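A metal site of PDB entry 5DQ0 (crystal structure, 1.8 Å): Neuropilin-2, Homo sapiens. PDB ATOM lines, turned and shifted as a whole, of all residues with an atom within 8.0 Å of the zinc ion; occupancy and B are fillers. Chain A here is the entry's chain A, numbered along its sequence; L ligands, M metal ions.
The backbone NH of Tyr 104 sits at hydrogen-bond distance from the backbone carbonyl oxygen of Leu 92. O of Tyr 104 lies within hydrogen-bond range of N of Lys 111, at 2.9 Å.
The side-chain hydroxyl (OH) of Tyr 104 is bound to the zinc ion (1.9 Å). The zinc ion is bound by ND1 of His 128, at 2.1 Å. A ring nitrogen (NE2) of His 106 binds the zinc ion (2.1 Å). The zinc ion is bound by a chlorine (CL1) of the ligand (2.1 Å). The zinc ion has four donor atoms within binding distance.
The nearest printed residue that does not touch the zinc ion is Leu 127 (4.8 Å).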
ATOM      1  N   LEU A  92      18.886  27.012  -7.497  1.00  0.00           N
ATOM      2  CA  LEU A  92      19.980  27.763  -6.981  1.00  0.00           C
ATOM      3  C   LEU A  92      19.538  29.218  -6.902  1.00  0.00           C
ATOM      4  O   LEU A  92      18.958  29.714  -7.859  1.00  0.00           O
ATOM      5  CB  LEU A  92      21.153  27.648  -7.933  1.00  0.00           C
ATOM      6  CG  LEU A  92      22.358  28.543  -7.848  1.00  0.00           C
ATOM      7  CD1 LEU A  92      23.167  28.321  -6.580  1.00  0.00           C
ATOM      8  CD2 LEU A  92      23.229  28.405  -9.090  1.00  0.00           C
ATOM      9  N   TYR A 104      18.408  31.360 -10.115  1.00  0.00           N
ATOM     10  CA  TYR A 104      19.165  31.125 -11.327  1.00  0.00           C
ATOM     11  C   TYR A 104      18.250  30.520 -12.420  1.00  0.00           C
ATOM     12  O   TYR A 104      17.534  29.542 -12.153  1.00  0.00           O
ATOM     13  CB  TYR A 104      20.360  30.210 -11.075  1.00  0.00           C
ATOM     14  CG  TYR A 104      21.184  29.908 -12.322  1.00  0.00           C
ATOM     15  CD1 TYR A 104      21.793  30.915 -13.043  1.00  0.00           C
ATOM     16  CD2 TYR A 104      21.350  28.613 -12.780  1.00  0.00           C
ATOM     17  CE1 TYR A 104      22.526  30.641 -14.199  1.00  0.00           C
ATOM     18  CE2 TYR A 104      22.070  28.309 -13.952  1.00  0.00           C
ATOM     19  CZ  TYR A 104      22.667  29.328 -14.658  1.00  0.00           C
ATOM     20  OH  TYR A 104      23.425  29.105 -15.797  1.00  0.00           O
ATOM     21  N   ARG A 105      18.268  31.163 -13.582  1.00  0.00           N
ATOM     22  CA  ARG A 105      17.362  30.781 -14.691  1.00  0.00           C
ATOM     23  C   ARG A 105      18.091  30.684 -16.008  1.00  0.00           C
ATOM     24  O   ARG A 105      19.146  31.238 -16.213  1.00  0.00           O
ATOM     25  CB  ARG A 105      16.152  31.702 -14.853  1.00  0.00           C
ATOM     26  CG  ARG A 105      16.365  33.131 -14.621  1.00  0.00           C
ATOM     27  CD  ARG A 105      15.034  33.893 -14.672  1.00  0.00           C
ATOM     28  NE  ARG A 105      15.406  35.274 -14.956  1.00  0.00           N
ATOM     29  CZ  ARG A 105      15.664  36.212 -14.038  1.00  0.00           C
ATOM     30  NH1 ARG A 105      15.540  35.989 -12.713  1.00  0.00           N
ATOM     31  NH2 ARG A 105      16.019  37.424 -14.459  1.00  0.00           N
ATOM     32  N   HIS A 106      17.474  29.929 -16.914  1.00  0.00           N
ATOM     33  CA  HIS A 106      17.776  29.957 -18.334  1.00  0.00           C
ATOM     34  C   HIS A 106      16.551  30.604 -19.005  1.00  0.00           C
ATOM     35  O   HIS A 106      15.444  30.033 -18.925  1.00  0.00           O
ATOM     36  CB  HIS A 106      17.932  28.506 -18.811  1.00  0.00           C
ATOM     37  CG  HIS A 106      19.174  27.844 -18.345  1.00  0.00           C
ATOM     38  ND1 HIS A 106      19.432  26.525 -18.626  1.00  0.00           N
ATOM     39  CD2 HIS A 106      20.272  28.308 -17.686  1.00  0.00           C
ATOM     40  CE1 HIS A 106      20.634  26.200 -18.161  1.00  0.00           C
ATOM     41  NE2 HIS A 106      21.147  27.262 -17.578  1.00  0.00           N
ATOM     42  N   LYS A 111      16.352  27.240 -13.466  1.00  0.00           N
ATOM     43  CA  LYS A 111      17.130  26.035 -13.711  1.00  0.00           C
ATOM     44  C   LYS A 111      16.925  25.034 -12.594  1.00  0.00           C
ATOM     45  O   LYS A 111      17.181  25.315 -11.432  1.00  0.00           O
ATOM     46  CB  LYS A 111      18.584  26.422 -13.926  1.00  0.00           C
ATOM     47  CG  LYS A 111      19.532  25.244 -14.082  1.00  0.00           C
ATOM     48  CD  LYS A 111      19.227  24.332 -15.259  1.00  0.00           C
ATOM     49  CE  LYS A 111      20.244  23.152 -15.275  1.00  0.00           C
ATOM     50  NZ  LYS A 111      19.952  22.269 -16.437  1.00  0.00           N
ATOM     51  N   PHE A 113      18.318  21.729 -11.179  1.00  0.00           N
ATOM     52  CA  PHE A 113      19.445  20.801 -11.263  1.00  0.00           C
ATOM     53  C   PHE A 113      18.988  19.416 -10.791  1.00  0.00           C
ATOM     54  O   PHE A 113      18.385  19.284  -9.756  1.00  0.00           O
ATOM     55  CB  PHE A 113      20.627  21.309 -10.418  1.00  0.00           C
ATOM     56  CG  PHE A 113      21.209  22.596 -10.933  1.00  0.00           C
ATOM     57  CD1 PHE A 113      22.244  22.587 -11.851  1.00  0.00           C
ATOM     58  CD2 PHE A 113      20.789  23.813 -10.430  1.00  0.00           C
ATOM     59  CE1 PHE A 113      22.835  23.747 -12.290  1.00  0.00           C
ATOM     60  CE2 PHE A 113      21.343  25.003 -10.915  1.00  0.00           C
ATOM     61  CZ  PHE A 113      22.353  24.975 -11.834  1.00  0.00           C
ATOM     62  N   LYS A 126      27.913  20.890 -13.636  1.00  0.00           N
ATOM     63  CA  LYS A 126      28.659  22.028 -14.124  1.00  0.00           C
ATOM     64  C   LYS A 126      27.678  23.075 -14.678  1.00  0.00           C
ATOM     65  O   LYS A 126      26.739  22.716 -15.368  1.00  0.00           O
ATOM     66  CB  LYS A 126      29.665  21.611 -15.193  1.00  0.00           C
ATOM     67  CG  LYS A 126      30.672  20.583 -14.671  1.00  0.00           C
ATOM     68  CD  LYS A 126      31.691  20.191 -15.749  1.00  0.00           C
ATOM     69  CE  LYS A 126      32.797  19.303 -15.160  1.00  0.00           C
ATOM     70  NZ  LYS A 126      33.548  18.587 -16.222  1.00  0.00           N
ATOM     71  N   LEU A 127      27.887  24.352 -14.396  1.00  0.00           N
ATOM     72  CA  LEU A 127      27.067  25.406 -14.995  1.00  0.00           C
ATOM     73  C   LEU A 127      27.469  25.635 -16.441  1.00  0.00           C
ATOM     74  O   LEU A 127      28.640  25.537 -16.795  1.00  0.00           O
ATOM     75  CB  LEU A 127      27.189  26.693 -14.195  1.00  0.00           C
ATOM     76  CG  LEU A 127      26.271  26.781 -12.949  1.00  0.00           C
ATOM     77  CD1 LEU A 127      26.648  25.798 -11.868  1.00  0.00           C
ATOM     78  CD2 LEU A 127      26.431  28.163 -12.389  1.00  0.00           C
ATOM     79  N   HIS A 128      26.521  26.035 -17.285  1.00  0.00           N
ATOM     80  CA  HIS A 128      26.813  26.189 -18.713  1.00  0.00           C
ATOM     81  C   HIS A 128      27.757  27.328 -18.989  1.00  0.00           C
ATOM     82  O   HIS A 128      28.418  27.350 -20.035  1.00  0.00           O
ATOM     83  CB  HIS A 128      25.509  26.329 -19.511  1.00  0.00           C
ATOM     84  CG  HIS A 128      24.981  27.711 -19.543  1.00  0.00           C
ATOM     85  ND1 HIS A 128      24.195  28.244 -18.549  1.00  0.00           N
ATOM     86  CD2 HIS A 128      25.164  28.697 -20.457  1.00  0.00           C
ATOM     87  CE1 HIS A 128      23.930  29.504 -18.841  1.00  0.00           C
ATOM     88  NE2 HIS A 128      24.498  29.801 -20.003  1.00  0.00           N
ATOM     89  N   ALA A 129      27.792  28.306 -18.100  1.00  0.00           N
ATOM     90  CA  ALA A 129      28.735  29.391 -18.134  1.00  0.00           C
ATOM     91  C   ALA A 129      28.941  29.879 -16.724  1.00  0.00           C
ATOM     92  O   ALA A 129      28.109  29.669 -15.863  1.00  0.00           O
ATOM     93  CB  ALA A 129      28.233  30.525 -19.036  1.00  0.00           C
ATOM     94  N   PRO A 130      30.080  30.504 -16.441  1.00  0.00           N
ATOM     95  CA  PRO A 130      30.291  30.873 -15.052  1.00  0.00           C
ATOM     96  C   PRO A 130      29.284  31.970 -14.563  1.00  0.00           C
ATOM     97  O   PRO A 130      28.812  32.803 -15.337  1.00  0.00           O
ATOM     98  CB  PRO A 130      31.716  31.383 -15.068  1.00  0.00           C
ATOM     99  CG  PRO A 130      32.353  30.838 -16.318  1.00  0.00           C
ATOM    100  CD  PRO A 130      31.243  30.814 -17.293  1.00  0.00           C
ATOM    101  N   LEU A 131      28.894  31.849 -13.309  1.00  0.00           N
ATOM    102  CA  LEU A 131      27.856  32.697 -12.741  1.00  0.00           C
ATOM    103  C   LEU A 131      28.459  33.543 -11.626  1.00  0.00           C
ATOM    104  O   LEU A 131      29.070  32.984 -10.718  1.00  0.00           O
ATOM    105  CB  LEU A 131      26.775  31.798 -12.202  1.00  0.00           C
ATOM    106  CG  LEU A 131      25.637  32.364 -11.333  1.00  0.00           C
ATOM    107  CD1 LEU A 131      24.909  33.420 -12.165  1.00  0.00           C
ATOM    108  CD2 LEU A 131      24.690  31.268 -10.838  1.00  0.00           C
HETATM  109 CL1  LIG L   1      23.589  25.612 -16.114  1.00  0.00          CL
HETATM  110 ZN    ZN M   1      23.133  27.554 -16.886  1.00  0.00          ZN
